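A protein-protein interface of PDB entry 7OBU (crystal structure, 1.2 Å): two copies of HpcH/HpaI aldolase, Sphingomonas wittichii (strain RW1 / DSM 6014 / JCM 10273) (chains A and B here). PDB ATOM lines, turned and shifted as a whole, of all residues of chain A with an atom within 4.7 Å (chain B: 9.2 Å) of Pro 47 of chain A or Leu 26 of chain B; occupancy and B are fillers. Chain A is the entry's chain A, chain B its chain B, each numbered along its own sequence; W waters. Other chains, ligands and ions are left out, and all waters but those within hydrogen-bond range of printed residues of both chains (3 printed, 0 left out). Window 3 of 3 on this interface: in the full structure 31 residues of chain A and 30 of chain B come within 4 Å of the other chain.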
ATOM      1  N   GLN A  21       7.182 -29.295   8.464  1.00  0.00           N
ATOM      2  CA  GLN A  21       5.739 -29.191   8.388  1.00  0.00           C
ATOM      3  C   GLN A  21       5.217 -27.934   9.042  1.00  0.00           C
ATOM      4  O   GLN A  21       4.010 -27.685   8.973  1.00  0.00           O
ATOM      5  CB  GLN A  21       5.114 -30.436   9.031  1.00  0.00           C
ATOM      6  CG  GLN A  21       5.360 -31.670   8.203  1.00  0.00           C
ATOM      7  CD  GLN A  21       5.188 -32.970   8.941  1.00  0.00           C
ATOM      8  OE1 GLN A  21       5.110 -33.012  10.164  1.00  0.00           O
ATOM      9  NE2 GLN A  21       5.107 -34.060   8.179  1.00  0.00           N
ATOM     10  N   LEU A  22       6.064 -27.172   9.713  1.00  0.00           N
ATOM     11  CA  LEU A  22       5.671 -25.930  10.351  1.00  0.00           C
ATOM     12  C   LEU A  22       5.984 -24.777   9.413  1.00  0.00           C
ATOM     13  O   LEU A  22       7.142 -24.643   8.984  1.00  0.00           O
ATOM     14  CB  LEU A  22       6.402 -25.743  11.671  1.00  0.00           C
ATOM     15  CG  LEU A  22       6.102 -26.831  12.702  1.00  0.00           C
ATOM     16  CD1 LEU A  22       6.937 -26.623  13.928  1.00  0.00           C
ATOM     17  CD2 LEU A  22       4.625 -26.895  13.083  1.00  0.00           C
ATOM     18  N   PRO A  23       5.022 -23.917   9.086  1.00  0.00           N
ATOM     19  CA  PRO A  23       5.339 -22.754   8.259  1.00  0.00           C
ATOM     20  C   PRO A  23       6.195 -21.743   9.003  1.00  0.00           C
ATOM     21  O   PRO A  23       6.161 -21.654  10.234  1.00  0.00           O
ATOM     22  CB  PRO A  23       3.964 -22.164   7.929  1.00  0.00           C
ATOM     23  CG  PRO A  23       3.040 -22.648   9.016  1.00  0.00           C
ATOM     24  CD  PRO A  23       3.590 -23.978   9.443  1.00  0.00           C
ATOM     25  N   SER A  46       0.802 -30.962   6.108  1.00  0.00           N
ATOM     26  CA  SER A  46       1.110 -29.735   6.819  1.00  0.00           C
ATOM     27  C   SER A  46       0.091 -28.691   6.388  1.00  0.00           C
ATOM     28  O   SER A  46      -0.627 -28.894   5.404  1.00  0.00           O
ATOM     29  CB  SER A  46       2.484 -29.206   6.399  1.00  0.00           C
ATOM     30  OG  SER A  46       2.356 -28.535   5.144  1.00  0.00           O
ATOM     31  N   PRO A  47       0.096 -27.539   7.022  1.00  0.00           N
ATOM     32  CA  PRO A  47      -0.741 -26.431   6.561  1.00  0.00           C
ATOM     33  C   PRO A  47       0.030 -25.442   5.700  1.00  0.00           C
ATOM     34  O   PRO A  47      -0.397 -24.291   5.560  1.00  0.00           O
ATOM     35  CB  PRO A  47      -1.177 -25.791   7.876  1.00  0.00           C
ATOM     36  CG  PRO A  47       0.035 -25.965   8.751  1.00  0.00           C
ATOM     37  CD  PRO A  47       0.639 -27.281   8.368  1.00  0.00           C
ATOM     38  N   ILE A  48       1.162 -25.855   5.133  1.00  0.00           N
ATOM     39  CA  ILE A  48       2.004 -24.944   4.359  1.00  0.00           C
ATOM     40  C   ILE A  48       1.466 -24.865   2.933  1.00  0.00           C
ATOM     41  O   ILE A  48       1.518 -25.852   2.182  1.00  0.00           O
ATOM     42  CB  ILE A  48       3.471 -25.376   4.361  1.00  0.00           C
ATOM     43  CG1 ILE A  48       4.021 -25.472   5.783  1.00  0.00           C
ATOM     44  CG2 ILE A  48       4.316 -24.399   3.523  1.00  0.00           C
ATOM     45  CD1 ILE A  48       5.413 -26.053   5.859  1.00  0.00           C
ATOM     46  N   ASP A  49       0.970 -23.685   2.546  1.00  0.00           N
ATOM     47  CA  ASP A  49       0.517 -23.401   1.191  1.00  0.00           C
ATOM     48  C   ASP A  49       1.594 -22.636   0.429  1.00  0.00           C
ATOM     49  O   ASP A  49       2.667 -22.334   0.949  1.00  0.00           O
ATOM     50  CB  ASP A  49      -0.794 -22.610   1.227  1.00  0.00           C
ATOM     51  CG  ASP A  49      -0.646 -21.243   1.881  1.00  0.00           C
ATOM     52  OD1 ASP A  49       0.280 -21.047   2.679  1.00  0.00           O
ATOM     53  OD2 ASP A  49      -1.481 -20.354   1.588  1.00  0.00           O
ATOM     54  N   GLN A  52       3.001 -19.399   1.976  1.00  0.00           N
ATOM     55  CA  GLN A  52       3.940 -19.611   3.070  1.00  0.00           C
ATOM     56  C   GLN A  52       5.223 -20.305   2.641  1.00  0.00           C
ATOM     57  O   GLN A  52       6.279 -20.061   3.245  1.00  0.00           O
ATOM     58  CB  GLN A  52       3.232 -20.356   4.186  1.00  0.00           C
ATOM     59  CG  GLN A  52       2.208 -19.444   4.828  1.00  0.00           C
ATOM     60  CD  GLN A  52       1.506 -20.053   5.996  1.00  0.00           C
ATOM     61  OE1 GLN A  52       1.759 -19.700   7.152  1.00  0.00           O
ATOM     62  NE2 GLN A  52       0.572 -20.930   5.709  1.00  0.00           N
ATOM     63  N   LEU A 235       7.918 -30.643  13.505  1.00  0.00           N
ATOM     64  CA  LEU A 235       6.849 -30.737  14.501  1.00  0.00           C
ATOM     65  C   LEU A 235       7.091 -31.894  15.468  1.00  0.00           C
ATOM     66  O   LEU A 235       6.942 -31.733  16.684  1.00  0.00           O
ATOM     67  CB  LEU A 235       5.478 -30.846  13.822  1.00  0.00           C
ATOM     68  CG  LEU A 235       4.294 -31.152  14.754  1.00  0.00           C
ATOM     69  CD1 LEU A 235       4.109 -30.039  15.771  1.00  0.00           C
ATOM     70  CD2 LEU A 235       3.020 -31.403  13.940  1.00  0.00           C
ATOM     71  N   LEU B  20       6.842 -19.589  22.952  1.00  0.00           N
ATOM     72  CA  LEU B  20       6.907 -19.674  21.500  1.00  0.00           C
ATOM     73  C   LEU B  20       7.508 -18.415  20.890  1.00  0.00           C
ATOM     74  O   LEU B  20       7.001 -17.307  21.096  1.00  0.00           O
ATOM     75  CB  LEU B  20       5.525 -19.891  20.893  1.00  0.00           C
ATOM     76  CG  LEU B  20       4.692 -21.014  21.498  1.00  0.00           C
ATOM     77  CD1 LEU B  20       3.362 -21.146  20.749  1.00  0.00           C
ATOM     78  CD2 LEU B  20       5.447 -22.324  21.494  1.00  0.00           C
ATOM     79  N   LEU B  22       8.300 -19.035  17.432  1.00  0.00           N
ATOM     80  CA  LEU B  22       7.987 -19.363  16.047  1.00  0.00           C
ATOM     81  C   LEU B  22       6.516 -19.113  15.770  1.00  0.00           C
ATOM     82  O   LEU B  22       5.662 -19.620  16.504  1.00  0.00           O
ATOM     83  CB  LEU B  22       8.307 -20.825  15.749  1.00  0.00           C
ATOM     84  CG  LEU B  22       9.772 -21.203  15.976  1.00  0.00           C
ATOM     85  CD1 LEU B  22       9.961 -22.693  15.800  1.00  0.00           C
ATOM     86  CD2 LEU B  22      10.668 -20.429  15.038  1.00  0.00           C
ATOM     87  N   PRO B  23       6.180 -18.349  14.735  1.00  0.00           N
ATOM     88  CA  PRO B  23       4.763 -18.124  14.420  1.00  0.00           C
ATOM     89  C   PRO B  23       4.107 -19.384  13.881  1.00  0.00           C
ATOM     90  O   PRO B  23       4.757 -20.268  13.323  1.00  0.00           O
ATOM     91  CB  PRO B  23       4.802 -17.050  13.322  1.00  0.00           C
ATOM     92  CG  PRO B  23       6.189 -17.207  12.693  1.00  0.00           C
ATOM     93  CD  PRO B  23       7.087 -17.643  13.812  1.00  0.00           C
ATOM     94  N   GLY B  24       2.792 -19.460  14.068  1.00  0.00           N
ATOM     95  CA  GLY B  24       1.992 -20.517  13.474  1.00  0.00           C
ATOM     96  C   GLY B  24       1.141 -21.224  14.506  1.00  0.00           C
ATOM     97  O   GLY B  24       1.451 -21.196  15.694  1.00  0.00           O
ATOM     98  N   THR B  25       0.070 -21.867  14.051  1.00  0.00           N
ATOM     99  CA  THR B  25      -0.908 -22.482  14.941  1.00  0.00           C
ATOM    100  C   THR B  25      -0.664 -23.947  15.260  1.00  0.00           C
ATOM    101  O   THR B  25      -1.216 -24.437  16.254  1.00  0.00           O
ATOM    102  CB  THR B  25      -2.314 -22.315  14.355  1.00  0.00           C
ATOM    103  OG1 THR B  25      -2.301 -22.733  12.990  1.00  0.00           O
ATOM    104  CG2 THR B  25      -2.777 -20.891  14.382  1.00  0.00           C
ATOM    105  N   LEU B  26       0.102 -24.662  14.443  1.00  0.00           N
ATOM    106  CA  LEU B  26       0.131 -26.114  14.582  1.00  0.00           C
ATOM    107  C   LEU B  26       0.967 -26.546  15.779  1.00  0.00           C
ATOM    108  O   LEU B  26       0.495 -27.315  16.616  1.00  0.00           O
ATOM    109  CB  LEU B  26       0.607 -26.764  13.288  1.00  0.00           C
ATOM    110  CG  LEU B  26       0.679 -28.289  13.303  1.00  0.00           C
ATOM    111  CD1 LEU B  26      -0.625 -28.944  13.680  1.00  0.00           C
ATOM    112  CD2 LEU B  26       1.077 -28.756  11.913  1.00  0.00           C
ATOM    113  N   HIS B  27       2.199 -26.040  15.895  1.00  0.00           N
ATOM    114  CA  HIS B  27       2.966 -26.337  17.099  1.00  0.00           C
ATOM    115  C   HIS B  27       2.357 -25.676  18.324  1.00  0.00           C
ATOM    116  O   HIS B  27       2.490 -26.204  19.436  1.00  0.00           O
ATOM    117  CB  HIS B  27       4.427 -25.934  16.933  1.00  0.00           C
ATOM    118  CG  HIS B  27       4.658 -24.460  16.871  1.00  0.00           C
ATOM    119  ND1 HIS B  27       3.952 -23.621  16.033  1.00  0.00           N
ATOM    120  CD2 HIS B  27       5.443 -23.666  17.633  1.00  0.00           C
ATOM    121  CE1 HIS B  27       4.346 -22.381  16.249  1.00  0.00           C
ATOM    122  NE2 HIS B  27       5.255 -22.380  17.206  1.00  0.00           N
ATOM    123  N   ALA B  28       1.667 -24.544  18.145  1.00  0.00           N
ATOM    124  CA  ALA B  28       1.066 -23.874  19.289  1.00  0.00           C
ATOM    125  C   ALA B  28       0.012 -24.771  19.913  1.00  0.00           C
ATOM    126  O   ALA B  28      -0.012 -24.974  21.128  1.00  0.00           O
ATOM    127  CB  ALA B  28       0.483 -22.529  18.867  1.00  0.00           C
ATOM    128  N   GLU B  29      -0.836 -25.376  19.078  1.00  0.00           N
ATOM    129  CA  GLU B  29      -1.853 -26.279  19.600  1.00  0.00           C
ATOM    130  C   GLU B  29      -1.210 -27.546  20.148  1.00  0.00           C
ATOM    131  O   GLU B  29      -1.604 -28.032  21.203  1.00  0.00           O
ATOM    132  CB  GLU B  29      -2.866 -26.644  18.510  1.00  0.00           C
ATOM    133  CG  GLU B  29      -4.008 -27.487  19.057  1.00  0.00           C
ATOM    134  CD  GLU B  29      -4.936 -28.053  18.004  1.00  0.00           C
ATOM    135  OE1 GLU B  29      -5.042 -27.492  16.887  1.00  0.00           O
ATOM    136  OE2 GLU B  29      -5.649 -29.033  18.348  1.00  0.00           O
ATOM    137  N   ALA B  30      -0.244 -28.098  19.424  1.00  0.00           N
ATOM    138  CA  ALA B  30       0.397 -29.330  19.869  1.00  0.00           C
ATOM    139  C   ALA B  30       1.034 -29.161  21.245  1.00  0.00           C
ATOM    140  O   ALA B  30       0.885 -30.022  22.116  1.00  0.00           O
ATOM    141  CB  ALA B  30       1.446 -29.762  18.844  1.00  0.00           C
ATOM    142  N   LEU B  31       1.726 -28.041  21.479  1.00  0.00           N
ATOM    143  CA  LEU B  31       2.374 -27.820  22.772  1.00  0.00           C
ATOM    144  C   LEU B  31       1.330 -27.530  23.838  1.00  0.00           C
ATOM    145  O   LEU B  31       1.472 -27.967  24.981  1.00  0.00           O
ATOM    146  CB  LEU B  31       3.451 -26.729  22.642  1.00  0.00           C
ATOM    147  CG  LEU B  31       4.866 -27.262  22.353  1.00  0.00           C
ATOM    148  CD1 LEU B  31       4.878 -28.181  21.156  1.00  0.00           C
ATOM    149  CD2 LEU B  31       5.865 -26.144  22.206  1.00  0.00           C
ATOM    150  N   ALA B  32       0.265 -26.802  23.484  1.00  0.00           N
ATOM    151  CA  ALA B  32      -0.799 -26.538  24.446  1.00  0.00           C
ATOM    152  C   ALA B  32      -1.449 -27.818  24.958  1.00  0.00           C
ATOM    153  O   ALA B  32      -1.946 -27.853  26.090  1.00  0.00           O
ATOM    154  CB  ALA B  32      -1.852 -25.630  23.814  1.00  0.00           C
ATOM    155  N   ARG B  33      -1.495 -28.856  24.128  1.00  0.00           N
ATOM    156  CA  ARG B  33      -2.091 -30.121  24.528  1.00  0.00           C
ATOM    157  C   ARG B  33      -1.172 -30.963  25.403  1.00  0.00           C
ATOM    158  O   ARG B  33      -1.622 -31.988  25.943  1.00  0.00           O
ATOM    159  CB  ARG B  33      -2.519 -30.910  23.293  1.00  0.00           C
ATOM    160  CG  ARG B  33      -3.730 -30.284  22.607  1.00  0.00           C
ATOM    161  CD  ARG B  33      -4.175 -31.082  21.425  1.00  0.00           C
ATOM    162  NE  ARG B  33      -5.339 -30.511  20.754  1.00  0.00           N
ATOM    163  CZ  ARG B  33      -6.605 -30.723  21.077  1.00  0.00           C
ATOM    164  NH1 ARG B  33      -6.941 -31.410  22.154  1.00  0.00           N
ATOM    165  NH2 ARG B  33      -7.561 -30.215  20.304  1.00  0.00           N
ATOM    166  N   GLN B  52      -0.033 -12.482  13.152  1.00  0.00           N
ATOM    167  CA  GLN B  52       0.264 -13.886  13.387  1.00  0.00           C
ATOM    168  C   GLN B  52      -0.077 -14.347  14.799  1.00  0.00           C
ATOM    169  O   GLN B  52      -0.363 -15.536  14.979  1.00  0.00           O
ATOM    170  CB  GLN B  52       1.702 -14.196  12.996  1.00  0.00           C
ATOM    171  CG  GLN B  52       1.930 -13.971  11.528  1.00  0.00           C
ATOM    172  CD  GLN B  52       3.344 -14.182  11.137  1.00  0.00           C
ATOM    173  OE1 GLN B  52       4.178 -13.294  11.306  1.00  0.00           O
ATOM    174  NE2 GLN B  52       3.634 -15.352  10.597  1.00  0.00           N
ATOM    175  N   PRO B  55      -4.334 -15.871  15.467  1.00  0.00           N
ATOM    176  CA  PRO B  55      -4.799 -17.267  15.387  1.00  0.00           C
ATOM    177  C   PRO B  55      -4.098 -18.185  16.381  1.00  0.00           C
ATOM    178  O   PRO B  55      -4.638 -19.230  16.755  1.00  0.00           O
ATOM    179  CB  PRO B  55      -4.513 -17.655  13.941  1.00  0.00           C
ATOM    180  CG  PRO B  55      -3.350 -16.716  13.532  1.00  0.00           C
ATOM    181  CD  PRO B  55      -3.654 -15.421  14.246  1.00  0.00           C
ATOM    182  N   MET B  56      -2.867 -17.866  16.783  1.00  0.00           N
ATOM    183  CA  MET B  56      -2.130 -18.694  17.748  1.00  0.00           C
ATOM    184  C   MET B  56      -2.848 -18.686  19.088  1.00  0.00           C
ATOM    185  O   MET B  56      -2.867 -19.705  19.783  1.00  0.00           O
ATOM    186  CB  MET B  56      -0.747 -18.052  17.880  1.00  0.00           C
ATOM    187  CG  MET B  56       0.154 -18.343  16.699  1.00  0.00           C
ATOM    188  SD  MET B  56       1.771 -17.525  16.817  1.00  0.00           S
ATOM    189  CE  MET B  56       2.575 -18.822  17.823  1.00  0.00           C
ATOM    190  N   ALA B  59      -5.567 -21.238  18.810  1.00  0.00           N
ATOM    191  CA  ALA B  59      -5.019 -22.590  18.783  1.00  0.00           C
ATOM    192  C   ALA B  59      -4.600 -23.063  20.170  1.00  0.00           C
ATOM    193  O   ALA B  59      -4.854 -24.219  20.553  1.00  0.00           O
ATOM    194  CB  ALA B  59      -3.834 -22.630  17.825  1.00  0.00           C
ATOM    195  N   ILE B  60      -3.977 -22.181  20.951  1.00  0.00           N
ATOM    196  CA  ILE B  60      -3.557 -22.546  22.304  1.00  0.00           C
ATOM    197  C   ILE B  60      -4.772 -22.810  23.175  1.00  0.00           C
ATOM    198  O   ILE B  60      -4.827 -23.798  23.913  1.00  0.00           O
ATOM    199  CB  ILE B  60      -2.661 -21.445  22.896  1.00  0.00           C
ATOM    200  CG1 ILE B  60      -1.304 -21.420  22.192  1.00  0.00           C
ATOM    201  CG2 ILE B  60      -2.473 -21.664  24.397  1.00  0.00           C
ATOM    202  CD1 ILE B  60      -0.569 -20.118  22.442  1.00  0.00           C
ATOM    203  N   GLY B  63      -6.210 -26.123  22.380  1.00  0.00           N
ATOM    204  CA  GLY B  63      -5.383 -27.185  22.897  1.00  0.00           C
ATOM    205  C   GLY B  63      -5.472 -27.381  24.397  1.00  0.00           C
ATOM    206  O   GLY B  63      -4.981 -28.404  24.882  1.00  0.00           O
ATOM    207  N   ASP B 234      10.521 -22.716  21.929  1.00  0.00           N
ATOM    208  CA  ASP B 234      10.333 -23.640  20.811  1.00  0.00           C
ATOM    209  C   ASP B 234      11.540 -23.688  19.880  1.00  0.00           C
ATOM    210  O   ASP B 234      12.013 -24.775  19.535  1.00  0.00           O
ATOM    211  CB  ASP B 234       9.033 -23.354  20.040  1.00  0.00           C
ATOM    212  CG  ASP B 234       8.875 -21.903  19.516  1.00  0.00           C
ATOM    213  OD1 ASP B 234       9.753 -21.044  19.724  1.00  0.00           O
ATOM    214  OD2 ASP B 234       7.798 -21.654  18.915  1.00  0.00           O
HETATM  215  O   HOH W   1       4.604 -22.839  12.308  1.00  0.00           O
HETATM  216  O   HOH W   2       7.531 -20.552  12.362  1.00  0.00           O
HETATM  217  O   HOH W   3       4.171 -19.350  10.419  1.00  0.00           O
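Pro 47 of chain A touches just one residue of chain B: Leu 26 (3.9 Å). No residue of chain B comes within 4 Å of Ser 46 of chain A. Of the printed residues of chain B, Leu 22 of chain A touches His 27. Printed residues of chain B within 4 Å of Leu 235 of chain A: Leu 26. Of the printed residues of chain A, Pro 23 of chain B touches Pro 23 (3.7 Å). Gly 24 of chain B touches none of the printed residues of chain A. Met 56 of chain B touches none of the printed residues of chain A. The nearest residue of chain B that does not touch Pro 47 of chain A is Thr 25 of chain B (5.8 Å). The nearest printed residue of chain A that does not touch Pro 23 of chain B is Leu 22 of chain A (6.0 Å).
Pro 23 of chain B touches its own counterpart, Pro 23 of chain A. Positions printed for both chains: 22, 23 and 52. Of the 4 pairs that touch across the chains among the printed residues, 1 has its exchanged pair printed and touching as well.
Printed residues of chain B that touch a printed residue of chain A: Pro 23, Leu 26 and His 27. Hydrophobic or aromatic side chains of chain A within 4 Å of the printed part of chain B: Leu 22, Pro 47 and Leu 235. Along chain A the printed residues that touch a printed residue of chain B span positions 22 to 235. Among the printed residues, 4 pairs touch across the chains. Among the printed residues, no Asp or Glu carboxylate lies within 4 Å of a Lys or Arg side-chain nitrogen of the other chain.
The backbone carbonyl oxygen of Leu 22 of chain B is in hydrogen-bond range of a ring nitrogen (NE2) of His 27 of chain B (2.9 Å). NE2 of His 27 of chain B lies within hydrogen-bond range of OD2 of Asp 234 of chain B (3.1 Å).
Water W2 lies within hydrogen-bond range of the backbone carbonyl oxygen (O) of Pro 23 of chain A and the backbone carbonyl oxygen (O) of Pro 23 of chain B. Water W1 lies within hydrogen-bond range of O of Pro 23 of chain B (2.8 Å) and O of Pro 23 of chain A (2.9 Å). Water W3 lies within hydrogen-bond range of the backbone carbonyl oxygen (O) of Pro 23 of chain A (3.1 Å) and the backbone carbonyl oxygen (O) of Pro 23 of chain B (3.1 Å).
Leu 22 of chain A touches His 27 of chain B (CD2 to N, 3.8 Å). Pro 23 of chain A touches Pro 23 of chain B (O to O, 3.7 Å). CD2 of Leu 26 of chain B touches CD of Pro 47 of chain A, 3.9 Å away. Leu 235 of chain A touches Leu 26 of chain B (CD2 to CD2, 3.9 Å).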
